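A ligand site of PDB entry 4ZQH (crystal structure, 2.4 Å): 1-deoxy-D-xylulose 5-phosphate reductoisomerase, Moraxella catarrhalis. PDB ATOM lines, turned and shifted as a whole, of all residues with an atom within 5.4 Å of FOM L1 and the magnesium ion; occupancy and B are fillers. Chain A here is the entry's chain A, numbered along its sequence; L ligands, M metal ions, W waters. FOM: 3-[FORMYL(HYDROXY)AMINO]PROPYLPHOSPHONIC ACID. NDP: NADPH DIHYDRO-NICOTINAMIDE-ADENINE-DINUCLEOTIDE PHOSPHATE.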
ATOM      1  N   LYS A 146      33.820 -15.529  18.895  1.00  0.00           N
ATOM      2  CA  LYS A 146      33.582 -16.951  18.638  1.00  0.00           C
ATOM      3  C   LYS A 146      33.404 -17.271  17.133  1.00  0.00           C
ATOM      4  O   LYS A 146      33.668 -18.395  16.678  1.00  0.00           O
ATOM      5  CB  LYS A 146      32.394 -17.468  19.457  1.00  0.00           C
ATOM      6  CG  LYS A 146      31.035 -17.025  18.959  1.00  0.00           C
ATOM      7  CD  LYS A 146      29.926 -17.365  19.939  1.00  0.00           C
ATOM      8  CE  LYS A 146      29.976 -16.443  21.166  1.00  0.00           C
ATOM      9  NZ  LYS A 146      28.846 -16.653  22.125  1.00  0.00           N
ATOM     10  N   ASP A 171      34.580 -16.440  26.222  1.00  0.00           N
ATOM     11  CA  ASP A 171      33.209 -16.908  26.137  1.00  0.00           C
ATOM     12  C   ASP A 171      32.910 -17.636  27.469  1.00  0.00           C
ATOM     13  O   ASP A 171      33.730 -18.437  27.990  1.00  0.00           O
ATOM     14  CB  ASP A 171      33.004 -17.813  24.896  1.00  0.00           C
ATOM     15  CG  ASP A 171      31.576 -17.755  24.356  1.00  0.00           C
ATOM     16  OD1 ASP A 171      30.734 -17.189  25.024  1.00  0.00           O
ATOM     17  OD2 ASP A 171      31.296 -18.262  23.249  1.00  0.00           O
ATOM     18  N   SER A 172      31.761 -17.316  28.045  1.00  0.00           N
ATOM     19  CA  SER A 172      31.427 -17.741  29.385  1.00  0.00           C
ATOM     20  C   SER A 172      31.466 -19.280  29.548  1.00  0.00           C
ATOM     21  O   SER A 172      32.071 -19.822  30.494  1.00  0.00           O
ATOM     22  CB  SER A 172      30.043 -17.179  29.738  1.00  0.00           C
ATOM     23  OG  SER A 172      29.669 -17.539  31.033  1.00  0.00           O
ATOM     24  N   GLU A 173      30.836 -19.971  28.606  1.00  0.00           N
ATOM     25  CA  GLU A 173      30.692 -21.404  28.684  1.00  0.00           C
ATOM     26  C   GLU A 173      32.042 -22.088  28.592  1.00  0.00           C
ATOM     27  O   GLU A 173      32.333 -23.028  29.327  1.00  0.00           O
ATOM     28  CB  GLU A 173      29.772 -21.916  27.585  1.00  0.00           C
ATOM     29  CG  GLU A 173      28.313 -21.460  27.724  1.00  0.00           C
ATOM     30  CD  GLU A 173      28.093 -20.042  27.251  1.00  0.00           C
ATOM     31  OE1 GLU A 173      26.963 -19.511  27.284  1.00  0.00           O
ATOM     32  OE2 GLU A 173      29.094 -19.482  26.826  1.00  0.00           O
ATOM     33  N   HIS A 174      32.867 -21.580  27.716  1.00  0.00           N
ATOM     34  CA  HIS A 174      34.151 -22.156  27.402  1.00  0.00           C
ATOM     35  C   HIS A 174      35.130 -21.824  28.503  1.00  0.00           C
ATOM     36  O   HIS A 174      36.064 -22.567  28.778  1.00  0.00           O
ATOM     37  CB  HIS A 174      34.625 -21.631  26.053  1.00  0.00           C
ATOM     38  CG  HIS A 174      33.662 -21.944  24.949  1.00  0.00           C
ATOM     39  ND1 HIS A 174      32.447 -21.311  24.825  1.00  0.00           N
ATOM     40  CD2 HIS A 174      33.697 -22.875  23.975  1.00  0.00           C
ATOM     41  CE1 HIS A 174      31.780 -21.812  23.801  1.00  0.00           C
ATOM     42  NE2 HIS A 174      32.514 -22.771  23.271  1.00  0.00           N
ATOM     43  N   THR A 205      25.598 -25.123  28.671  1.00  0.00           N
ATOM     44  CA  THR A 205      24.343 -24.560  29.155  1.00  0.00           C
ATOM     45  C   THR A 205      23.866 -23.412  28.243  1.00  0.00           C
ATOM     46  O   THR A 205      24.655 -22.645  27.710  1.00  0.00           O
ATOM     47  CB  THR A 205      24.516 -24.060  30.593  1.00  0.00           C
ATOM     48  OG1 THR A 205      25.815 -23.458  30.744  1.00  0.00           O
ATOM     49  CG2 THR A 205      24.397 -25.229  31.546  1.00  0.00           C
ATOM     50  N   ALA A 206      22.554 -23.314  28.087  1.00  0.00           N
ATOM     51  CA  ALA A 206      21.935 -22.320  27.220  1.00  0.00           C
ATOM     52  C   ALA A 206      20.744 -21.763  27.959  1.00  0.00           C
ATOM     53  O   ALA A 206      19.981 -22.527  28.510  1.00  0.00           O
ATOM     54  CB  ALA A 206      21.457 -22.988  25.936  1.00  0.00           C
ATOM     55  N   SER A 207      20.560 -20.450  27.931  1.00  0.00           N
ATOM     56  CA  SER A 207      19.429 -19.825  28.626  1.00  0.00           C
ATOM     57  C   SER A 207      18.109 -20.164  27.965  1.00  0.00           C
ATOM     58  O   SER A 207      17.071 -20.076  28.601  1.00  0.00           O
ATOM     59  CB  SER A 207      19.553 -18.309  28.635  1.00  0.00           C
ATOM     60  OG  SER A 207      19.272 -17.766  27.350  1.00  0.00           O
ATOM     61  N   GLY A 208      18.156 -20.528  26.691  1.00  0.00           N
ATOM     62  CA  GLY A 208      16.960 -20.704  25.885  1.00  0.00           C
ATOM     63  C   GLY A 208      16.382 -19.359  25.476  1.00  0.00           C
ATOM     64  O   GLY A 208      15.261 -19.311  24.988  1.00  0.00           O
ATOM     65  N   GLY A 209      17.149 -18.263  25.640  1.00  0.00           N
ATOM     66  CA  GLY A 209      16.742 -16.937  25.197  1.00  0.00           C
ATOM     67  C   GLY A 209      15.356 -16.502  25.625  1.00  0.00           C
ATOM     68  O   GLY A 209      14.685 -17.209  26.361  1.00  0.00           O
ATOM     69  N   HIS A 230      17.479  -9.532  26.533  1.00  0.00           N
ATOM     70  CA  HIS A 230      17.683 -10.839  27.123  1.00  0.00           C
ATOM     71  C   HIS A 230      17.410 -10.736  28.624  1.00  0.00           C
ATOM     72  O   HIS A 230      17.829  -9.763  29.256  1.00  0.00           O
ATOM     73  CB  HIS A 230      19.115 -11.316  26.883  1.00  0.00           C
ATOM     74  CG  HIS A 230      19.314 -12.765  27.175  1.00  0.00           C
ATOM     75  ND1 HIS A 230      19.413 -13.267  28.449  1.00  0.00           N
ATOM     76  CD2 HIS A 230      19.379 -13.840  26.344  1.00  0.00           C
ATOM     77  CE1 HIS A 230      19.530 -14.583  28.401  1.00  0.00           C
ATOM     78  NE2 HIS A 230      19.518 -14.951  27.134  1.00  0.00           N
ATOM     79  N   TRP A 233      21.224 -11.248  30.539  1.00  0.00           N
ATOM     80  CA  TRP A 233      22.506 -10.764  30.008  1.00  0.00           C
ATOM     81  C   TRP A 233      22.265  -9.460  29.258  1.00  0.00           C
ATOM     82  O   TRP A 233      21.230  -9.289  28.621  1.00  0.00           O
ATOM     83  CB  TRP A 233      23.085 -11.742  28.993  1.00  0.00           C
ATOM     84  CG  TRP A 233      23.581 -13.014  29.474  1.00  0.00           C
ATOM     85  CD1 TRP A 233      22.964 -14.207  29.380  1.00  0.00           C
ATOM     86  CD2 TRP A 233      24.839 -13.268  30.087  1.00  0.00           C
ATOM     87  NE1 TRP A 233      23.739 -15.196  29.918  1.00  0.00           N
ATOM     88  CE2 TRP A 233      24.902 -14.641  30.354  1.00  0.00           C
ATOM     89  CE3 TRP A 233      25.914 -12.466  30.455  1.00  0.00           C
ATOM     90  CZ2 TRP A 233      26.003 -15.219  30.991  1.00  0.00           C
ATOM     91  CZ3 TRP A 233      27.009 -13.043  31.046  1.00  0.00           C
ATOM     92  CH2 TRP A 233      27.033 -14.410  31.327  1.00  0.00           C
ATOM     93  N   MET A 235      24.096  -7.586  26.212  1.00  0.00           N
ATOM     94  CA  MET A 235      25.157  -7.882  25.270  1.00  0.00           C
ATOM     95  C   MET A 235      25.028  -7.084  23.977  1.00  0.00           C
ATOM     96  O   MET A 235      24.147  -6.264  23.825  1.00  0.00           O
ATOM     97  CB  MET A 235      25.146  -9.370  24.934  1.00  0.00           C
ATOM     98  CG  MET A 235      24.857 -10.283  26.091  1.00  0.00           C
ATOM     99  SD  MET A 235      24.591 -11.983  25.567  1.00  0.00           S
ATOM    100  CE  MET A 235      22.865 -11.866  25.060  1.00  0.00           C
ATOM    101  N   ILE A 239      24.814 -11.174  19.154  1.00  0.00           N
ATOM    102  CA  ILE A 239      24.779 -12.282  20.084  1.00  0.00           C
ATOM    103  C   ILE A 239      23.430 -12.295  20.804  1.00  0.00           C
ATOM    104  O   ILE A 239      22.945 -13.334  21.188  1.00  0.00           O
ATOM    105  CB  ILE A 239      25.951 -12.241  21.096  1.00  0.00           C
ATOM    106  CG1 ILE A 239      26.019 -13.531  21.896  1.00  0.00           C
ATOM    107  CG2 ILE A 239      25.838 -11.080  22.060  1.00  0.00           C
ATOM    108  CD1 ILE A 239      27.384 -13.781  22.517  1.00  0.00           C
ATOM    109  N   SER A 243      21.132 -15.537  20.639  1.00  0.00           N
ATOM    110  CA  SER A 243      20.654 -16.165  21.859  1.00  0.00           C
ATOM    111  C   SER A 243      19.194 -16.524  21.770  1.00  0.00           C
ATOM    112  O   SER A 243      18.801 -17.612  22.195  1.00  0.00           O
ATOM    113  CB  SER A 243      20.875 -15.219  23.018  1.00  0.00           C
ATOM    114  OG  SER A 243      20.202 -15.711  24.143  1.00  0.00           O
ATOM    115  N   ASN A 248      23.466 -19.104  18.953  1.00  0.00           N
ATOM    116  CA  ASN A 248      24.617 -18.836  19.788  1.00  0.00           C
ATOM    117  C   ASN A 248      25.244 -20.121  20.338  1.00  0.00           C
ATOM    118  O   ASN A 248      26.475 -20.262  20.373  1.00  0.00           O
ATOM    119  CB  ASN A 248      24.244 -17.869  20.942  1.00  0.00           C
ATOM    120  CG  ASN A 248      25.441 -17.513  21.815  1.00  0.00           C
ATOM    121  OD1 ASN A 248      26.490 -17.081  21.341  1.00  0.00           O
ATOM    122  ND2 ASN A 248      25.278 -17.700  23.124  1.00  0.00           N
ATOM    123  N   LYS A 249      24.381 -21.037  20.777  1.00  0.00           N
ATOM    124  CA  LYS A 249      24.863 -22.342  21.286  1.00  0.00           C
ATOM    125  C   LYS A 249      25.464 -23.182  20.168  1.00  0.00           C
ATOM    126  O   LYS A 249      26.498 -23.833  20.340  1.00  0.00           O
ATOM    127  CB  LYS A 249      23.736 -23.083  22.001  1.00  0.00           C
ATOM    128  CG  LYS A 249      24.193 -23.773  23.284  1.00  0.00           C
ATOM    129  CD  LYS A 249      24.965 -22.864  24.232  1.00  0.00           C
ATOM    130  CE  LYS A 249      24.288 -21.508  24.409  1.00  0.00           C
ATOM    131  NZ  LYS A 249      24.924 -20.699  25.463  1.00  0.00           N
ATOM    132  N   GLU A 252      28.773 -21.862  19.686  1.00  0.00           N
ATOM    133  CA  GLU A 252      29.507 -22.286  20.867  1.00  0.00           C
ATOM    134  C   GLU A 252      29.880 -23.769  20.761  1.00  0.00           C
ATOM    135  O   GLU A 252      31.011 -24.164  21.129  1.00  0.00           O
ATOM    136  CB  GLU A 252      28.725 -21.927  22.119  1.00  0.00           C
ATOM    137  CG  GLU A 252      28.797 -20.416  22.393  1.00  0.00           C
ATOM    138  CD  GLU A 252      27.982 -19.962  23.602  1.00  0.00           C
ATOM    139  OE1 GLU A 252      27.456 -20.821  24.347  1.00  0.00           O
ATOM    140  OE2 GLU A 252      27.825 -18.735  23.783  1.00  0.00           O
ATOM    141  N   SER A 275      20.703 -19.073  34.028  1.00  0.00           N
ATOM    142  CA  SER A 275      22.024 -18.565  33.653  1.00  0.00           C
ATOM    143  C   SER A 275      22.981 -18.446  34.847  1.00  0.00           C
ATOM    144  O   SER A 275      23.850 -17.606  34.870  1.00  0.00           O
ATOM    145  CB  SER A 275      21.930 -17.234  32.890  1.00  0.00           C
ATOM    146  OG  SER A 275      21.314 -17.383  31.626  1.00  0.00           O
ATOM    147  N   MET A 297      29.976 -10.986  32.377  1.00  0.00           N
ATOM    148  CA  MET A 297      31.202 -11.360  31.680  1.00  0.00           C
ATOM    149  C   MET A 297      32.466 -10.880  32.356  1.00  0.00           C
ATOM    150  O   MET A 297      33.548 -11.213  31.920  1.00  0.00           O
ATOM    151  CB  MET A 297      31.188 -10.829  30.250  1.00  0.00           C
ATOM    152  CG  MET A 297      30.073 -11.402  29.355  1.00  0.00           C
ATOM    153  SD  MET A 297      30.098 -13.197  29.262  1.00  0.00           S
ATOM    154  CE  MET A 297      31.749 -13.521  28.643  1.00  0.00           C
HETATM  155  O2  FOM L   1      27.123 -16.520  25.116  1.00  0.00           O
HETATM  156  N1  FOM L   1      26.919 -15.811  26.280  1.00  0.00           N
HETATM  157  C1  FOM L   1      27.810 -15.735  27.179  1.00  0.00           C
HETATM  158  O1  FOM L   1      28.844 -16.362  27.058  1.00  0.00           O
HETATM  159  C2  FOM L   1      25.583 -15.269  26.475  1.00  0.00           C
HETATM  160  C3  FOM L   1      24.756 -16.554  26.628  1.00  0.00           C
HETATM  161  C4  FOM L   1      23.297 -16.373  26.252  1.00  0.00           C
HETATM  162  PA1 FOM L   1      22.604 -17.993  25.852  1.00  0.00           P
HETATM  163  OP1 FOM L   1      22.696 -18.903  27.004  1.00  0.00           O
HETATM  164  OP2 FOM L   1      21.066 -17.742  25.534  1.00  0.00           O
HETATM  165  OP3 FOM L   1      23.457 -18.680  24.670  1.00  0.00           O
HETATM  166  PA  NDP L   2      29.323  -5.443  20.111  1.00  0.00           P
HETATM  167  O1A NDP L   2      28.343  -5.300  18.974  1.00  0.00           O
HETATM  168  O2A NDP L   2      29.056  -4.765  21.428  1.00  0.00           O
HETATM  169  O5B NDP L   2      30.815  -4.990  19.770  1.00  0.00           O
HETATM  170  C5B NDP L   2      31.448  -5.242  18.534  1.00  0.00           C
HETATM  171  C4B NDP L   2      32.863  -4.649  18.551  1.00  0.00           C
HETATM  172  O4B NDP L   2      33.559  -4.927  17.309  1.00  0.00           O
HETATM  173  C3B NDP L   2      32.796  -3.132  18.676  1.00  0.00           C
HETATM  174  O3B NDP L   2      33.989  -2.627  19.261  1.00  0.00           O
HETATM  175  C2B NDP L   2      32.655  -2.692  17.218  1.00  0.00           C
HETATM  176  O2B NDP L   2      32.985  -1.313  17.051  1.00  0.00           O
HETATM  177  C1B NDP L   2      33.592  -3.711  16.537  1.00  0.00           C
HETATM  178  N9A NDP L   2      33.208  -3.986  15.112  1.00  0.00           N
HETATM  179  C8A NDP L   2      31.954  -4.183  14.641  1.00  0.00           C
HETATM  180  N7A NDP L   2      31.979  -4.381  13.315  1.00  0.00           N
HETATM  181  C5A NDP L   2      33.273  -4.327  12.929  1.00  0.00           C
HETATM  182  C6A NDP L   2      33.988  -4.462  11.648  1.00  0.00           C
HETATM  183  N6A NDP L   2      33.273  -4.725  10.528  1.00  0.00           N
HETATM  184  N1A NDP L   2      35.328  -4.332  11.641  1.00  0.00           N
HETATM  185  C2A NDP L   2      35.995  -4.090  12.788  1.00  0.00           C
HETATM  186  N3A NDP L   2      35.410  -3.934  13.982  1.00  0.00           N
HETATM  187  C4A NDP L   2      34.066  -4.047  14.101  1.00  0.00           C
HETATM  188  O3  NDP L   2      29.421  -7.044  20.292  1.00  0.00           O
HETATM  189  PN  NDP L   2      29.840  -7.846  21.611  1.00  0.00           P
HETATM  190  O1N NDP L   2      30.945  -7.149  22.415  1.00  0.00           O
HETATM  191  O2N NDP L   2      28.543  -8.296  22.197  1.00  0.00           O
HETATM  192  O5D NDP L   2      30.482  -9.154  21.012  1.00  0.00           O
HETATM  193  C5D NDP L   2      31.880  -9.168  20.762  1.00  0.00           C
HETATM  194  C4D NDP L   2      32.271 -10.612  20.561  1.00  0.00           C
HETATM  195  O4D NDP L   2      32.210 -11.293  21.810  1.00  0.00           O
HETATM  196  C3D NDP L   2      31.326 -11.346  19.645  1.00  0.00           C
HETATM  197  O3D NDP L   2      32.177 -12.205  18.874  1.00  0.00           O
HETATM  198  C2D NDP L   2      30.428 -12.138  20.564  1.00  0.00           C
HETATM  199  O2D NDP L   2      29.984 -13.339  19.918  1.00  0.00           O
HETATM  200  C1D NDP L   2      31.344 -12.407  21.759  1.00  0.00           C
HETATM  201  N1N NDP L   2      30.675 -12.540  23.054  1.00  0.00           N
HETATM  202  C2N NDP L   2      30.045 -11.508  23.620  1.00  0.00           C
HETATM  203  C3N NDP L   2      29.389 -11.596  24.848  1.00  0.00           C
HETATM  204  C7N NDP L   2      28.729 -10.390  25.491  1.00  0.00           C
HETATM  205  O7N NDP L   2      28.545  -9.317  24.918  1.00  0.00           O
HETATM  206  N7N NDP L   2      28.354 -10.499  26.755  1.00  0.00           N
HETATM  207  C4N NDP L   2      29.379 -12.903  25.595  1.00  0.00           C
HETATM  208  C5N NDP L   2      30.092 -13.944  24.882  1.00  0.00           C
HETATM  209  C6N NDP L   2      30.722 -13.719  23.661  1.00  0.00           C
HETATM  210  P2B NDP L   2      31.793  -0.199  17.049  1.00  0.00           P
HETATM  211  O1X NDP L   2      30.820  -0.692  18.081  1.00  0.00           O
HETATM  212  O2X NDP L   2      32.570   1.039  17.430  1.00  0.00           O
HETATM  213  O3X NDP L   2      31.185  -0.242  15.671  1.00  0.00           O
HETATM  214 MG    MG M   1      28.764 -17.850  25.517  1.00  0.00          MG
HETATM  215  O   HOH W   1      22.168 -19.883  22.487  1.00  0.00           O
HETATM  216  O   HOH W   2      19.804 -19.577  24.086  1.00  0.00           O
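The side-chain amino group (NZ) of Lys 249 is in salt-bridge range of an oxygen (OP3) of FOM L1, 2.6 Å away. N of Ser 172 lies close to O1 of FOM L1, at 3.2 Å. The side-chain hydroxyl of Ser 243 sits at hydrogen-bond distance from an oxygen (OP2) of FOM L1, 2.6 Å away. NZ of Lys 146 lies close to O2 of FOM L1 (3.5 Å). OG of Ser 207 sits at hydrogen-bond distance from OP2 of FOM L1, 2.6 Å away. ND2 of Asn 248 sits at hydrogen-bond distance from OP3 of FOM L1, 2.6 Å away. The backbone NH (N) of Ser 207 is in hydrogen-bond range of an oxygen (OP1) of FOM L1 (2.8 Å).
The side-chain amide nitrogen (ND2) of Asn 248 lies close to the side-chain carboxylate (OE2) of Glu 252, at 2.8 Å. The side-chain amino group (NZ) of Lys 249 lies within salt-bridge range of the side-chain carboxylate (OE1) of Glu 173, 3.0 Å away. O of Glu 252 is in hydrogen-bond range of NE2 of His 174, 3.0 Å away. A ring nitrogen (NE2) of His 230 sits at hydrogen-bond distance from the side-chain hydroxyl (OG) of Ser 207, 2.8 Å away. OE2 of Glu 252 lies close to NZ of Lys 146 (2.9 Å). The side-chain amide oxygen (OD1) of Asn 248 sits at hydrogen-bond distance from the side-chain amino group (NZ) of Lys 146 (2.5 Å). NZ of Lys 249 sits at hydrogen-bond distance from O of Thr 205 (3.0 Å). ND1 of His 230 sits at hydrogen-bond distance from N of Trp 233 (3.4 Å).
Ala 206 touches FOM L1. Gly 209 touches FOM L1. NE2 of His 230 touches OP2 of FOM L1, at 3.6 Å. Trp 233 touches FOM L1 (NE1 to C3, 3.7 Å). SD of Met 235 touches C2 of FOM L1, 3.6 Å away. Ile 239 touches FOM L1 (CD1 to O2, 3.8 Å). Hydrophobic or aromatic side chains within 4 Å of FOM L1: Trp 233, Met 235 and Ile 239. Within 4 Å of FOM L1: Lys 146, Asp 171, Ser 172, Glu 173, Ala 206, Ser 207, Gly 209, His 230, Trp 233, Met 235, Ile 239, Ser 243, Asn 248, Lys 249 and Glu 252.
Lys 146 touches the magnesium ion (NZ to MG, 3.6 Å). N of Ser 172 touches the magnesium ion (3.96 Å).
OE2 of Glu 173 binds the magnesium ion. OD1 of Asp 171 binds the magnesium ion, at 2.1 Å. O1 of FOM L1 is bound to the magnesium ion (2.1 Å). The magnesium ion is bound by O2 of FOM L1, 2.2 Å away. The magnesium ion is bound by the side-chain carboxylate (OE2) of Glu 252 (2.2 Å). The magnesium ion has five donor atoms within binding distance.
Water W2 lies within hydrogen-bond range of an oxygen (OP2) of FOM L1 (2.7 Å), the backbone carbonyl oxygen (O) of Ser 243 (2.9 Å), the backbone NH (N) of Gly 208 (3.2 Å) and the backbone NH (N) of Gly 209 (3.3 Å). Water W1 bridges an oxygen (OP3) of FOM L1 (2.8 Å) and the backbone NH of Lys 249 (3.0 Å).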
